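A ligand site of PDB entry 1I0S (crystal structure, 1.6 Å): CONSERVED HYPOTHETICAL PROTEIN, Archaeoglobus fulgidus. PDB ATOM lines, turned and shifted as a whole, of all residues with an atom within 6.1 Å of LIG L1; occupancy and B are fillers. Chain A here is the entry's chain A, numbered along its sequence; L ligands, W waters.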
ATOM      1  N   LEU A  13     -39.036 -27.866   9.058  1.00  0.00           N
ATOM      2  CA  LEU A  13     -37.607 -28.065   9.335  1.00  0.00           C
ATOM      3  C   LEU A  13     -37.338 -29.473   8.830  1.00  0.00           C
ATOM      4  O   LEU A  13     -38.069 -30.421   9.132  1.00  0.00           O
ATOM      5  CB  LEU A  13     -37.251 -27.886  10.810  1.00  0.00           C
ATOM      6  CG  LEU A  13     -35.745 -27.604  10.967  1.00  0.00           C
ATOM      7  CD1 LEU A  13     -35.371 -26.276  10.312  1.00  0.00           C
ATOM      8  CD2 LEU A  13     -35.369 -27.615  12.462  1.00  0.00           C
ATOM      9  N   CYS A  25     -24.084 -37.272   2.572  1.00  0.00           N
ATOM     10  CA  CYS A  25     -24.163 -35.897   3.051  1.00  0.00           C
ATOM     11  C   CYS A  25     -25.588 -35.587   3.502  1.00  0.00           C
ATOM     12  O   CYS A  25     -26.560 -36.063   2.909  1.00  0.00           O
ATOM     13  CB  CYS A  25     -23.798 -34.920   1.930  1.00  0.00           C
ATOM     14  SG  CYS A  25     -22.084 -34.987   1.375  1.00  0.00           S
ATOM     15  N   GLY A  26     -25.700 -34.779   4.539  1.00  0.00           N
ATOM     16  CA  GLY A  26     -27.006 -34.365   5.003  1.00  0.00           C
ATOM     17  C   GLY A  26     -26.850 -33.027   5.708  1.00  0.00           C
ATOM     18  O   GLY A  26     -25.826 -32.766   6.334  1.00  0.00           O
ATOM     19  N   GLN A  27     -27.866 -32.175   5.610  1.00  0.00           N
ATOM     20  CA  GLN A  27     -27.833 -30.891   6.291  1.00  0.00           C
ATOM     21  C   GLN A  27     -29.241 -30.541   6.731  1.00  0.00           C
ATOM     22  O   GLN A  27     -30.213 -31.056   6.198  1.00  0.00           O
ATOM     23  CB  GLN A  27     -27.347 -29.783   5.352  1.00  0.00           C
ATOM     24  CG  GLN A  27     -28.243 -29.578   4.106  1.00  0.00           C
ATOM     25  CD  GLN A  27     -28.025 -28.232   3.487  1.00  0.00           C
ATOM     26  OE1 GLN A  27     -28.600 -27.219   3.926  1.00  0.00           O
ATOM     27  NE2 GLN A  27     -27.186 -28.185   2.470  1.00  0.00           N
ATOM     28  N   ILE A  28     -29.351 -29.681   7.725  1.00  0.00           N
ATOM     29  CA  ILE A  28     -30.669 -29.213   8.116  1.00  0.00           C
ATOM     30  C   ILE A  28     -31.023 -28.098   7.097  1.00  0.00           C
ATOM     31  O   ILE A  28     -30.148 -27.388   6.604  1.00  0.00           O
ATOM     32  CB  ILE A  28     -30.643 -28.569   9.525  1.00  0.00           C
ATOM     33  CG1 ILE A  28     -30.376 -29.639  10.587  1.00  0.00           C
ATOM     34  CG2 ILE A  28     -31.963 -27.796   9.763  1.00  0.00           C
ATOM     35  CD1 ILE A  28     -31.503 -30.640  10.776  1.00  0.00           C
ATOM     36  N   ALA A  29     -32.298 -28.011   6.732  1.00  0.00           N
ATOM     37  CA  ALA A  29     -32.732 -26.932   5.855  1.00  0.00           C
ATOM     38  C   ALA A  29     -34.139 -26.575   6.232  1.00  0.00           C
ATOM     39  O   ALA A  29     -34.922 -27.450   6.606  1.00  0.00           O
ATOM     40  CB  ALA A  29     -32.684 -27.370   4.378  1.00  0.00           C
ATOM     41  N   ASN A  30     -34.447 -25.281   6.189  1.00  0.00           N
ATOM     42  CA  ASN A  30     -35.827 -24.898   6.400  1.00  0.00           C
ATOM     43  C   ASN A  30     -36.429 -24.576   5.037  1.00  0.00           C
ATOM     44  O   ASN A  30     -37.642 -24.593   4.875  1.00  0.00           O
ATOM     45  CB  ASN A  30     -35.951 -23.691   7.388  1.00  0.00           C
ATOM     46  CG  ASN A  30     -35.335 -22.368   6.869  1.00  0.00           C
ATOM     47  OD1 ASN A  30     -34.612 -22.321   5.887  1.00  0.00           O
ATOM     48  ND2 ASN A  30     -35.633 -21.296   7.580  1.00  0.00           N
ATOM     49  N   THR A  31     -35.575 -24.351   4.028  1.00  0.00           N
ATOM     50  CA  THR A  31     -36.045 -23.961   2.695  1.00  0.00           C
ATOM     51  C   THR A  31     -36.336 -25.139   1.784  1.00  0.00           C
ATOM     52  O   THR A  31     -35.547 -25.480   0.883  1.00  0.00           O
ATOM     53  CB  THR A  31     -35.022 -23.025   2.017  1.00  0.00           C
ATOM     54  OG1 THR A  31     -34.609 -22.026   2.964  1.00  0.00           O
ATOM     55  CG2 THR A  31     -35.656 -22.339   0.822  1.00  0.00           C
ATOM     56  N   VAL A  32     -37.480 -25.758   2.032  1.00  0.00           N
ATOM     57  CA  VAL A  32     -37.953 -26.924   1.276  1.00  0.00           C
ATOM     58  C   VAL A  32     -39.441 -26.694   1.019  1.00  0.00           C
ATOM     59  O   VAL A  32     -40.199 -26.474   1.965  1.00  0.00           O
ATOM     60  CB  VAL A  32     -37.799 -28.228   2.106  1.00  0.00           C
ATOM     61  CG1 VAL A  32     -38.328 -29.397   1.306  1.00  0.00           C
ATOM     62  CG2 VAL A  32     -36.311 -28.463   2.436  1.00  0.00           C
ATOM     63  N   CYS A  45     -33.312 -25.269  -1.261  1.00  0.00           N
ATOM     64  CA  CYS A  45     -32.352 -24.187  -1.540  1.00  0.00           C
ATOM     65  C   CYS A  45     -31.157 -24.391  -0.611  1.00  0.00           C
ATOM     66  O   CYS A  45     -31.281 -24.223   0.597  1.00  0.00           O
ATOM     67  CB  CYS A  45     -33.009 -22.825  -1.306  1.00  0.00           C
ATOM     68  SG  CYS A  45     -32.054 -21.503  -2.075  1.00  0.00           S
ATOM     69  N   LEU A  46     -30.012 -24.729  -1.196  1.00  0.00           N
ATOM     70  CA  LEU A  46     -28.805 -25.052  -0.438  1.00  0.00           C
ATOM     71  C   LEU A  46     -27.636 -24.130  -0.717  1.00  0.00           C
ATOM     72  O   LEU A  46     -27.331 -23.810  -1.864  1.00  0.00           O
ATOM     73  CB  LEU A  46     -28.378 -26.501  -0.757  1.00  0.00           C
ATOM     74  CG  LEU A  46     -29.491 -27.557  -0.774  1.00  0.00           C
ATOM     75  CD1 LEU A  46     -28.885 -28.924  -1.156  1.00  0.00           C
ATOM     76  CD2 LEU A  46     -30.181 -27.629   0.592  1.00  0.00           C
ATOM     77  N   ASN A  47     -26.950 -23.732   0.355  1.00  0.00           N
ATOM     78  CA  ASN A  47     -25.818 -22.825   0.249  1.00  0.00           C
ATOM     79  C   ASN A  47     -24.685 -23.526  -0.530  1.00  0.00           C
ATOM     80  O   ASN A  47     -24.393 -24.701  -0.275  1.00  0.00           O
ATOM     81  CB  ASN A  47     -25.357 -22.438   1.662  1.00  0.00           C
ATOM     82  CG  ASN A  47     -24.338 -21.329   1.669  1.00  0.00           C
ATOM     83  OD1 ASN A  47     -23.289 -21.437   1.043  1.00  0.00           O
ATOM     84  ND2 ASN A  47     -24.646 -20.245   2.389  1.00  0.00           N
ATOM     85  N   GLU A  49     -21.671 -23.354  -0.230  1.00  0.00           N
ATOM     86  CA  GLU A  49     -20.557 -23.751   0.640  1.00  0.00           C
ATOM     87  C   GLU A  49     -20.780 -25.122   1.286  1.00  0.00           C
ATOM     88  O   GLU A  49     -19.852 -25.702   1.850  1.00  0.00           O
ATOM     89  CB  GLU A  49     -20.390 -22.746   1.783  1.00  0.00           C
ATOM     90  CG  GLU A  49     -19.899 -21.369   1.402  1.00  0.00           C
ATOM     91  CD  GLU A  49     -19.645 -20.494   2.626  1.00  0.00           C
ATOM     92  OE1 GLU A  49     -19.190 -21.045   3.657  1.00  0.00           O
ATOM     93  OE2 GLU A  49     -19.871 -19.270   2.568  1.00  0.00           O
ATOM     94  N   ASN A  50     -21.996 -25.638   1.188  1.00  0.00           N
ATOM     95  CA  ASN A  50     -22.328 -26.883   1.880  1.00  0.00           C
ATOM     96  C   ASN A  50     -21.913 -28.144   1.157  1.00  0.00           C
ATOM     97  O   ASN A  50     -22.015 -28.216  -0.055  1.00  0.00           O
ATOM     98  CB  ASN A  50     -23.845 -26.984   2.128  1.00  0.00           C
ATOM     99  CG  ASN A  50     -24.373 -25.878   3.015  1.00  0.00           C
ATOM    100  OD1 ASN A  50     -25.590 -25.733   3.168  1.00  0.00           O
ATOM    101  ND2 ASN A  50     -23.472 -25.096   3.619  1.00  0.00           N
ATOM    102  N   ASP A  51     -21.477 -29.145   1.922  1.00  0.00           N
ATOM    103  CA  ASP A  51     -21.106 -30.414   1.320  1.00  0.00           C
ATOM    104  C   ASP A  51     -22.342 -31.044   0.672  1.00  0.00           C
ATOM    105  O   ASP A  51     -22.250 -31.673  -0.384  1.00  0.00           O
ATOM    106  CB  ASP A  51     -20.512 -31.361   2.374  1.00  0.00           C
ATOM    107  CG  ASP A  51     -19.079 -30.989   2.767  1.00  0.00           C
ATOM    108  OD1 ASP A  51     -18.678 -31.357   3.897  1.00  0.00           O
ATOM    109  OD2 ASP A  51     -18.356 -30.340   1.956  1.00  0.00           O
ATOM    110  N   THR A  52     -23.519 -30.867   1.278  1.00  0.00           N
ATOM    111  CA  THR A  52     -24.723 -31.464   0.721  1.00  0.00           C
ATOM    112  C   THR A  52     -25.053 -30.812  -0.629  1.00  0.00           C
ATOM    113  O   THR A  52     -25.507 -31.490  -1.552  1.00  0.00           O
ATOM    114  CB  THR A  52     -25.925 -31.358   1.709  1.00  0.00           C
ATOM    115  OG1 THR A  52     -25.569 -31.935   2.975  1.00  0.00           O
ATOM    116  CG2 THR A  52     -27.133 -32.118   1.159  1.00  0.00           C
ATOM    117  N   HIS A  53     -24.835 -29.505  -0.731  1.00  0.00           N
ATOM    118  CA  HIS A  53     -25.055 -28.795  -1.995  1.00  0.00           C
ATOM    119  C   HIS A  53     -24.222 -29.457  -3.106  1.00  0.00           C
ATOM    120  O   HIS A  53     -24.712 -29.742  -4.188  1.00  0.00           O
ATOM    121  CB  HIS A  53     -24.649 -27.320  -1.860  1.00  0.00           C
ATOM    122  CG  HIS A  53     -24.441 -26.623  -3.175  1.00  0.00           C
ATOM    123  ND1 HIS A  53     -25.388 -25.774  -3.726  1.00  0.00           N
ATOM    124  CD2 HIS A  53     -23.408 -26.653  -4.045  1.00  0.00           C
ATOM    125  CE1 HIS A  53     -24.927 -25.300  -4.877  1.00  0.00           C
ATOM    126  NE2 HIS A  53     -23.725 -25.820  -5.097  1.00  0.00           N
ATOM    127  N   ILE A  76     -30.692 -32.098  15.644  1.00  0.00           N
ATOM    128  CA  ILE A  76     -30.690 -30.981  14.713  1.00  0.00           C
ATOM    129  C   ILE A  76     -29.248 -30.477  14.547  1.00  0.00           C
ATOM    130  O   ILE A  76     -28.804 -30.211  13.436  1.00  0.00           O
ATOM    131  CB  ILE A  76     -31.622 -29.861  15.234  1.00  0.00           C
ATOM    132  CG1 ILE A  76     -33.078 -30.338  15.158  1.00  0.00           C
ATOM    133  CG2 ILE A  76     -31.400 -28.559  14.419  1.00  0.00           C
ATOM    134  CD1 ILE A  76     -34.097 -29.406  15.879  1.00  0.00           C
ATOM    135  N   PHE A  79     -26.756 -32.467  12.259  1.00  0.00           N
ATOM    136  CA  PHE A  79     -26.851 -32.154  10.833  1.00  0.00           C
ATOM    137  C   PHE A  79     -26.729 -30.693  10.438  1.00  0.00           C
ATOM    138  O   PHE A  79     -26.350 -30.395   9.307  1.00  0.00           O
ATOM    139  CB  PHE A  79     -28.172 -32.670  10.262  1.00  0.00           C
ATOM    140  CG  PHE A  79     -28.232 -34.160  10.139  1.00  0.00           C
ATOM    141  CD1 PHE A  79     -28.782 -34.939  11.144  1.00  0.00           C
ATOM    142  CD2 PHE A  79     -27.716 -34.786   9.008  1.00  0.00           C
ATOM    143  CE1 PHE A  79     -28.836 -36.324  11.027  1.00  0.00           C
ATOM    144  CE2 PHE A  79     -27.761 -36.173   8.879  1.00  0.00           C
ATOM    145  CZ  PHE A  79     -28.330 -36.954   9.887  1.00  0.00           C
ATOM    146  N   GLY A  80     -26.981 -29.785  11.367  1.00  0.00           N
ATOM    147  CA  GLY A  80     -26.964 -28.387  11.000  1.00  0.00           C
ATOM    148  C   GLY A  80     -25.825 -27.487  11.464  1.00  0.00           C
ATOM    149  O   GLY A  80     -25.825 -26.309  11.129  1.00  0.00           O
ATOM    150  N   PHE A  81     -24.883 -28.035  12.215  1.00  0.00           N
ATOM    151  CA  PHE A  81     -23.777 -27.224  12.704  1.00  0.00           C
ATOM    152  C   PHE A  81     -22.402 -27.806  12.477  1.00  0.00           C
ATOM    153  O   PHE A  81     -21.462 -27.524  13.223  1.00  0.00           O
ATOM    154  CB  PHE A  81     -23.958 -26.903  14.204  1.00  0.00           C
ATOM    155  CG  PHE A  81     -25.100 -25.947  14.470  1.00  0.00           C
ATOM    156  CD1 PHE A  81     -26.277 -26.403  15.046  1.00  0.00           C
ATOM    157  CD2 PHE A  81     -25.010 -24.616  14.099  1.00  0.00           C
ATOM    158  CE1 PHE A  81     -27.373 -25.541  15.245  1.00  0.00           C
ATOM    159  CE2 PHE A  81     -26.088 -23.744  14.293  1.00  0.00           C
ATOM    160  CZ  PHE A  81     -27.264 -24.210  14.872  1.00  0.00           C
ATOM    161  N   ARG A  82     -22.270 -28.635  11.431  1.00  0.00           N
ATOM    162  CA  ARG A  82     -20.975 -29.202  11.066  1.00  0.00           C
ATOM    163  C   ARG A  82     -21.064 -29.675   9.615  1.00  0.00           C
ATOM    164  O   ARG A  82     -22.154 -29.768   9.072  1.00  0.00           O
ATOM    165  CB  ARG A  82     -20.613 -30.369  11.983  1.00  0.00           C
ATOM    166  CG  ARG A  82     -21.550 -31.565  11.883  1.00  0.00           C
ATOM    167  CD  ARG A  82     -21.582 -32.341  13.204  1.00  0.00           C
ATOM    168  NE  ARG A  82     -22.381 -31.639  14.209  1.00  0.00           N
ATOM    169  CZ  ARG A  82     -22.189 -31.725  15.518  1.00  0.00           C
ATOM    170  NH1 ARG A  82     -21.197 -32.476  15.989  1.00  0.00           N
ATOM    171  NH2 ARG A  82     -22.970 -31.028  16.356  1.00  0.00           N
ATOM    172  N   LYS A  83     -19.913 -29.967   9.008  1.00  0.00           N
ATOM    173  CA  LYS A  83     -19.895 -30.410   7.609  1.00  0.00           C
ATOM    174  C   LYS A  83     -19.865 -31.916   7.477  1.00  0.00           C
ATOM    175  O   LYS A  83     -19.160 -32.603   8.229  1.00  0.00           O
ATOM    176  CB  LYS A  83     -18.682 -29.840   6.888  1.00  0.00           C
ATOM    177  CG  LYS A  83     -18.717 -28.319   6.768  1.00  0.00           C
ATOM    178  CD  LYS A  83     -17.530 -27.804   5.991  1.00  0.00           C
ATOM    179  CE  LYS A  83     -17.673 -26.322   5.728  1.00  0.00           C
ATOM    180  NZ  LYS A  83     -18.732 -26.069   4.698  1.00  0.00           N
ATOM    181  N   SER A  84     -20.624 -32.431   6.504  1.00  0.00           N
ATOM    182  CA  SER A  84     -20.713 -33.868   6.258  1.00  0.00           C
ATOM    183  C   SER A  84     -19.381 -34.567   5.981  1.00  0.00           C
ATOM    184  O   SER A  84     -19.231 -35.737   6.305  1.00  0.00           O
ATOM    185  CB  SER A  84     -21.632 -34.155   5.066  1.00  0.00           C
ATOM    186  OG  SER A  84     -22.966 -33.760   5.320  1.00  0.00           O
ATOM    187  N   SER A  85     -18.466 -33.856   5.338  1.00  0.00           N
ATOM    188  CA  SER A  85     -17.158 -34.418   4.991  1.00  0.00           C
ATOM    189  C   SER A  85     -16.200 -34.408   6.169  1.00  0.00           C
ATOM    190  O   SER A  85     -15.134 -35.027   6.104  1.00  0.00           O
ATOM    191  CB  SER A  85     -16.526 -33.620   3.857  1.00  0.00           C
ATOM    192  OG  SER A  85     -16.222 -32.272   4.240  1.00  0.00           O
ATOM    193  N   LYS A  89     -21.995 -37.775  10.045  1.00  0.00           N
ATOM    194  CA  LYS A  89     -23.353 -37.455  10.475  1.00  0.00           C
ATOM    195  C   LYS A  89     -24.292 -38.642  10.507  1.00  0.00           C
ATOM    196  O   LYS A  89     -25.221 -38.670  11.315  1.00  0.00           O
ATOM    197  CB  LYS A  89     -23.961 -36.372   9.578  1.00  0.00           C
ATOM    198  CG  LYS A  89     -23.301 -35.007   9.695  1.00  0.00           C
ATOM    199  CD  LYS A  89     -23.915 -34.022   8.729  1.00  0.00           C
ATOM    200  CE  LYS A  89     -23.354 -32.609   8.951  1.00  0.00           C
ATOM    201  NZ  LYS A  89     -23.896 -31.583   8.007  1.00  0.00           N
ATOM    202  N   HIS A 126     -26.596 -19.370  -2.995  1.00  0.00           N
ATOM    203  CA  HIS A 126     -27.259 -20.661  -2.964  1.00  0.00           C
ATOM    204  C   HIS A 126     -27.679 -21.138  -4.331  1.00  0.00           C
ATOM    205  O   HIS A 126     -27.780 -20.363  -5.293  1.00  0.00           O
ATOM    206  CB  HIS A 126     -28.574 -20.601  -2.148  1.00  0.00           C
ATOM    207  CG  HIS A 126     -28.420 -20.384  -0.666  1.00  0.00           C
ATOM    208  ND1 HIS A 126     -27.814 -19.267  -0.123  1.00  0.00           N
ATOM    209  CD2 HIS A 126     -28.886 -21.108   0.378  1.00  0.00           C
ATOM    210  CE1 HIS A 126     -27.904 -19.329   1.196  1.00  0.00           C
ATOM    211  NE2 HIS A 126     -28.554 -20.440   1.525  1.00  0.00           N
ATOM    212  N   TYR A 147     -40.040 -24.164  11.701  1.00  0.00           N
ATOM    213  CA  TYR A 147     -38.866 -23.349  11.953  1.00  0.00           C
ATOM    214  C   TYR A 147     -39.166 -22.410  13.129  1.00  0.00           C
ATOM    215  O   TYR A 147     -38.282 -22.090  13.924  1.00  0.00           O
ATOM    216  CB  TYR A 147     -38.504 -22.560  10.680  1.00  0.00           C
ATOM    217  CG  TYR A 147     -37.254 -21.707  10.757  1.00  0.00           C
ATOM    218  CD1 TYR A 147     -36.011 -22.257  11.129  1.00  0.00           C
ATOM    219  CD2 TYR A 147     -37.296 -20.337  10.466  1.00  0.00           C
ATOM    220  CE1 TYR A 147     -34.877 -21.460  11.224  1.00  0.00           C
ATOM    221  CE2 TYR A 147     -36.164 -19.542  10.552  1.00  0.00           C
ATOM    222  CZ  TYR A 147     -34.949 -20.103  10.930  1.00  0.00           C
ATOM    223  OH  TYR A 147     -33.834 -19.304  11.038  1.00  0.00           O
ATOM    224  N   TYR A 150     -38.668 -24.323  16.238  1.00  0.00           N
ATOM    225  CA  TYR A 150     -37.234 -24.422  16.502  1.00  0.00           C
ATOM    226  C   TYR A 150     -36.738 -23.141  17.167  1.00  0.00           C
ATOM    227  O   TYR A 150     -35.899 -23.206  18.047  1.00  0.00           O
ATOM    228  CB  TYR A 150     -36.474 -24.671  15.191  1.00  0.00           C
ATOM    229  CG  TYR A 150     -35.007 -24.303  15.239  1.00  0.00           C
ATOM    230  CD1 TYR A 150     -34.069 -25.181  15.798  1.00  0.00           C
ATOM    231  CD2 TYR A 150     -34.558 -23.092  14.726  1.00  0.00           C
ATOM    232  CE1 TYR A 150     -32.714 -24.833  15.835  1.00  0.00           C
ATOM    233  CE2 TYR A 150     -33.225 -22.738  14.753  1.00  0.00           C
ATOM    234  CZ  TYR A 150     -32.296 -23.617  15.314  1.00  0.00           C
ATOM    235  OH  TYR A 150     -30.972 -23.238  15.358  1.00  0.00           O
HETATM  236  N1  LIG L   1     -28.586 -24.272   4.939  1.00  0.00           N
HETATM  237  C1  LIG L   1     -29.058 -24.125   3.672  1.00  0.00           C
HETATM  238  O1  LIG L   1     -28.330 -24.167   2.700  1.00  0.00           O
HETATM  239  N2  LIG L   1     -30.454 -23.956   3.480  1.00  0.00           N
HETATM  240  C2  LIG L   1     -31.401 -23.902   4.478  1.00  0.00           C
HETATM  241  O2  LIG L   1     -32.605 -23.758   4.205  1.00  0.00           O
HETATM  242  C3  LIG L   1     -30.886 -24.045   5.842  1.00  0.00           C
HETATM  243  N3  LIG L   1     -31.712 -24.010   6.901  1.00  0.00           N
HETATM  244  C4  LIG L   1     -31.178 -24.216   8.163  1.00  0.00           C
HETATM  245  C5  LIG L   1     -32.049 -24.232   9.333  1.00  0.00           C
HETATM  246  C6  LIG L   1     -31.613 -24.473  10.605  1.00  0.00           C
HETATM  247  C7  LIG L   1     -32.549 -24.463  11.818  1.00  0.00           C
HETATM  248  C8  LIG L   1     -30.178 -24.789  10.816  1.00  0.00           C
HETATM  249  C9  LIG L   1     -29.644 -25.112  12.198  1.00  0.00           C
HETATM  250  C10 LIG L   1     -29.321 -24.752   9.705  1.00  0.00           C
HETATM  251  C11 LIG L   1     -29.764 -24.468   8.393  1.00  0.00           C
HETATM  252  N4  LIG L   1     -28.932 -24.418   7.251  1.00  0.00           N
HETATM  253  C12 LIG L   1     -29.425 -24.242   5.980  1.00  0.00           C
HETATM  254  C13 LIG L   1     -27.470 -24.603   7.397  1.00  0.00           C
HETATM  255  C14 LIG L   1     -26.963 -26.017   7.163  1.00  0.00           C
HETATM  256  O3  LIG L   1     -27.756 -27.007   7.803  1.00  0.00           O
HETATM  257  C15 LIG L   1     -25.552 -26.095   7.715  1.00  0.00           C
HETATM  258  O4  LIG L   1     -24.698 -25.090   7.074  1.00  0.00           O
HETATM  259  C16 LIG L   1     -24.919 -27.453   7.597  1.00  0.00           C
HETATM  260  O5  LIG L   1     -23.751 -27.479   8.457  1.00  0.00           O
HETATM  261  C17 LIG L   1     -24.449 -27.801   6.210  1.00  0.00           C
HETATM  262  O6  LIG L   1     -23.897 -29.142   6.243  1.00  0.00           O
HETATM  263  P1  LIG L   1     -23.116 -29.758   4.983  1.00  0.00           P
HETATM  264  O7  LIG L   1     -21.912 -28.901   4.724  1.00  0.00           O
HETATM  265  O8  LIG L   1     -24.089 -29.792   3.843  1.00  0.00           O
HETATM  266  O9  LIG L   1     -22.739 -31.156   5.506  1.00  0.00           O
HETATM  267  P1  LG2 L   2     -29.645 -17.257  12.709  1.00  0.00           P
HETATM  268  O1  LG2 L   2     -30.020 -17.111  11.265  1.00  0.00           O
HETATM  269  O2  LG2 L   2     -28.185 -17.449  12.919  1.00  0.00           O
HETATM  270  O3  LG2 L   2     -30.205 -15.951  13.492  1.00  0.00           O
HETATM  271  C1  LG2 L   2     -29.334 -15.307  14.504  1.00  0.00           C
HETATM  272  C2  LG2 L   2     -30.331 -14.643  15.533  1.00  0.00           C
HETATM  273  O4  LG2 L   2     -31.270 -13.812  14.808  1.00  0.00           O
HETATM  274  C3  LG2 L   2     -31.193 -15.666  16.324  1.00  0.00           C
HETATM  275  O5  LG2 L   2     -30.425 -16.215  17.356  1.00  0.00           O
HETATM  276  C4  LG2 L   2     -32.322 -14.647  16.780  1.00  0.00           C
HETATM  277  O6  LG2 L   2     -31.895 -13.648  17.674  1.00  0.00           O
HETATM  278  C5  LG2 L   2     -32.541 -13.964  15.440  1.00  0.00           C
HETATM  279  N1  LG2 L   2     -33.419 -14.642  14.509  1.00  0.00           N
HETATM  280  C6  LG2 L   2     -33.125 -15.052  13.222  1.00  0.00           C
HETATM  281  N2  LG2 L   2     -34.124 -15.636  12.615  1.00  0.00           N
HETATM  282  C7  LG2 L   2     -35.120 -15.611  13.543  1.00  0.00           C
HETATM  283  C8  LG2 L   2     -36.464 -16.099  13.476  1.00  0.00           C
HETATM  284  N3  LG2 L   2     -36.886 -16.674  12.360  1.00  0.00           N
HETATM  285  N4  LG2 L   2     -37.257 -15.935  14.594  1.00  0.00           N
HETATM  286  C9  LG2 L   2     -36.714 -15.310  15.715  1.00  0.00           C
HETATM  287  N5  LG2 L   2     -35.482 -14.825  15.849  1.00  0.00           N
HETATM  288  C10 LG2 L   2     -34.730 -15.014  14.721  1.00  0.00           C
HETATM  289  O7  LG2 L   2     -30.456 -18.408  13.327  1.00  0.00           O
HETATM  290  P2  LG2 L   2     -30.656 -19.986  13.262  1.00  0.00           P
HETATM  291  O8  LG2 L   2     -31.958 -20.345  12.653  1.00  0.00           O
HETATM  292  O9  LG2 L   2     -30.363 -20.675  14.553  1.00  0.00           O
HETATM  293  O10 LG2 L   2     -29.473 -20.387  12.201  1.00  0.00           O
HETATM  294  C11 LG2 L   2     -28.612 -21.505  12.494  1.00  0.00           C
HETATM  295  C12 LG2 L   2     -27.682 -21.651  11.272  1.00  0.00           C
HETATM  296  O11 LG2 L   2     -28.494 -21.785  10.093  1.00  0.00           O
HETATM  297  C13 LG2 L   2     -26.771 -20.429  11.038  1.00  0.00           C
HETATM  298  O12 LG2 L   2     -25.487 -20.917  10.615  1.00  0.00           O
HETATM  299  C14 LG2 L   2     -27.579 -19.653   9.928  1.00  0.00           C
HETATM  300  O13 LG2 L   2     -26.696 -18.841   9.152  1.00  0.00           O
HETATM  301  C15 LG2 L   2     -28.162 -20.812   9.101  1.00  0.00           C
HETATM  302  N6  LG2 L   2     -29.443 -20.560   8.369  1.00  0.00           N
HETATM  303  C16 LG2 L   2     -29.377 -20.693   6.964  1.00  0.00           C
HETATM  304  C17 LG2 L   2     -30.582 -20.512   6.258  1.00  0.00           C
HETATM  305  C18 LG2 L   2     -30.504 -20.678   4.704  1.00  0.00           C
HETATM  306  O14 LG2 L   2     -31.564 -20.618   4.060  1.00  0.00           O
HETATM  307  N7  LG2 L   2     -29.273 -20.935   4.183  1.00  0.00           N
HETATM  308  C19 LG2 L   2     -31.875 -20.211   6.860  1.00  0.00           C
HETATM  309  C20 LG2 L   2     -31.782 -20.119   8.306  1.00  0.00           C
HETATM  310  C21 LG2 L   2     -30.653 -20.275   9.057  1.00  0.00           C
HETATM  311  P3  LG2 L   2     -32.175 -13.873  19.334  1.00  0.00           P
HETATM  312  O15 LG2 L   2     -31.183 -12.830  19.793  1.00  0.00           O
HETATM  313  O16 LG2 L   2     -33.618 -13.495  19.451  1.00  0.00           O
HETATM  314  O17 LG2 L   2     -31.860 -15.256  19.624  1.00  0.00           O
HETATM  315  O   HOH W   1     -21.685 -25.577   7.919  1.00  0.00           O
HETATM  316  O   HOH W   2     -21.361 -26.382   5.261  1.00  0.00           O
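Water W2 lies within hydrogen-bond range of an oxygen (O7) of LIG L1, the side-chain amino group (NZ) of Lys 83 and the side-chain amide nitrogen (ND2) of Asn 50.
A ring nitrogen (ND1) of His 53 is in hydrogen-bond range of the backbone carbonyl oxygen of Leu 46, 3.3 Å away. The side-chain hydroxyl (OG) of Ser 85 sits at hydrogen-bond distance from the side-chain carboxylate (OD1) of Asp 51, 2.6 Å away. OG1 of Thr 52 lies close to N of Gly 26, at 3.2 Å. The side-chain amino group (NZ) of Lys 89 lies within hydrogen-bond range of the backbone carbonyl oxygen (O) of Phe 79 (3.0 Å). The side-chain sulfur (SG) of Cys 25 sits at hydrogen-bond distance from the backbone carbonyl oxygen (O) of Asp 51, at 3.8 Å. OD1 of Asn 50 is in hydrogen-bond range of NE2 of Gln 27, 3.0 Å away. The side-chain amide oxygen (OD1) of Asn 47 is in hydrogen-bond range of the backbone NH (N) of Glu 49 (2.8 Å). The side-chain hydroxyl (OG) of Ser 84 sits at hydrogen-bond distance from the backbone NH (N) of Gly 26, at 3.0 Å.
Leu 13 touches LIG L1. Gly 26 touches LIG L1 (O to O9, 3.6 Å). Ala 29 touches LIG L1. CA of Leu 46 touches O1 of LIG L1, at 3.3 Å. O of Phe 79 touches C16 of LIG L1 (3.7 Å). Gly 80 touches LIG L1. Phe 81 touches LIG L1 (CZ to C9, 3.7 Å). Lys 83 touches LIG L1. CD2 of His 126 touches O1 of LIG L1 (3.9 Å). Tyr 147 touches LIG L1 (CE1 to C7, 3.8 Å). Tyr 150 touches LIG L1.
An oxygen (O2) of LIG L1 lies within hydrogen-bond range of the backbone NH of Thr 31. OE1 of Gln 27 sits close to N1 of LIG L1 (3.1 Å). The backbone NH (N) of Asp 51 lies within hydrogen-bond range of an oxygen (O7) of LIG L1, 2.8 Å away. OG1 of Thr 31 sits at hydrogen-bond distance from O2 of LIG L1 (2.9 Å). The side-chain amino group (NZ) of Lys 89 lies within salt-bridge range of an oxygen (O9) of LIG L1 (2.8 Å). The side-chain hydroxyl (OH) of Tyr 150 sits at hydrogen-bond distance from an oxygen (O9) of LG2 L2 (2.8 Å). N of Asn 30 is in hydrogen-bond range of N3 of LIG L1. OD1 of Asn 50 sits close to O1 of LIG L1 (3.2 Å). O of Ile 28 is in hydrogen-bond range of O3 of LIG L1, at 2.7 Å. An oxygen (O9) of LIG L1 is in hydrogen-bond range of the side-chain hydroxyl of Ser 84 (2.6 Å). An oxygen (O9) of LIG L1 lies within hydrogen-bond range of the backbone NH of Ser 84 (2.7 Å). N7 of LG2 L2 sits at hydrogen-bond distance from NE2 of His 126. O3 of LIG L1 sits at hydrogen-bond distance from N of Ile 28 (3.1 Å). An oxygen (O8) of LG2 L2 lies within hydrogen-bond range of the side-chain hydroxyl (OH) of Tyr 147. O of Arg 82 is in hydrogen-bond range of O5 of LIG L1, at 2.9 Å. The backbone NH of Thr 52 sits at hydrogen-bond distance from an oxygen (O8) of LIG L1 (2.8 Å). An oxygen (O2) of LIG L1 sits close to the side-chain amide oxygen of Asn 30, at 3.0 Å. The side-chain hydroxyl (OG1) of Thr 52 sits at hydrogen-bond distance from an oxygen (O8) of LIG L1 (2.7 Å). O1 of LIG L1 is in hydrogen-bond range of N of Asn 47. O of Cys 45 lies within hydrogen-bond range of N2 of LIG L1 (3.0 Å).
A nitrogen (N7) of LG2 L2 sits close to a nitrogen (N1) of LIG L1 (3.5 Å).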
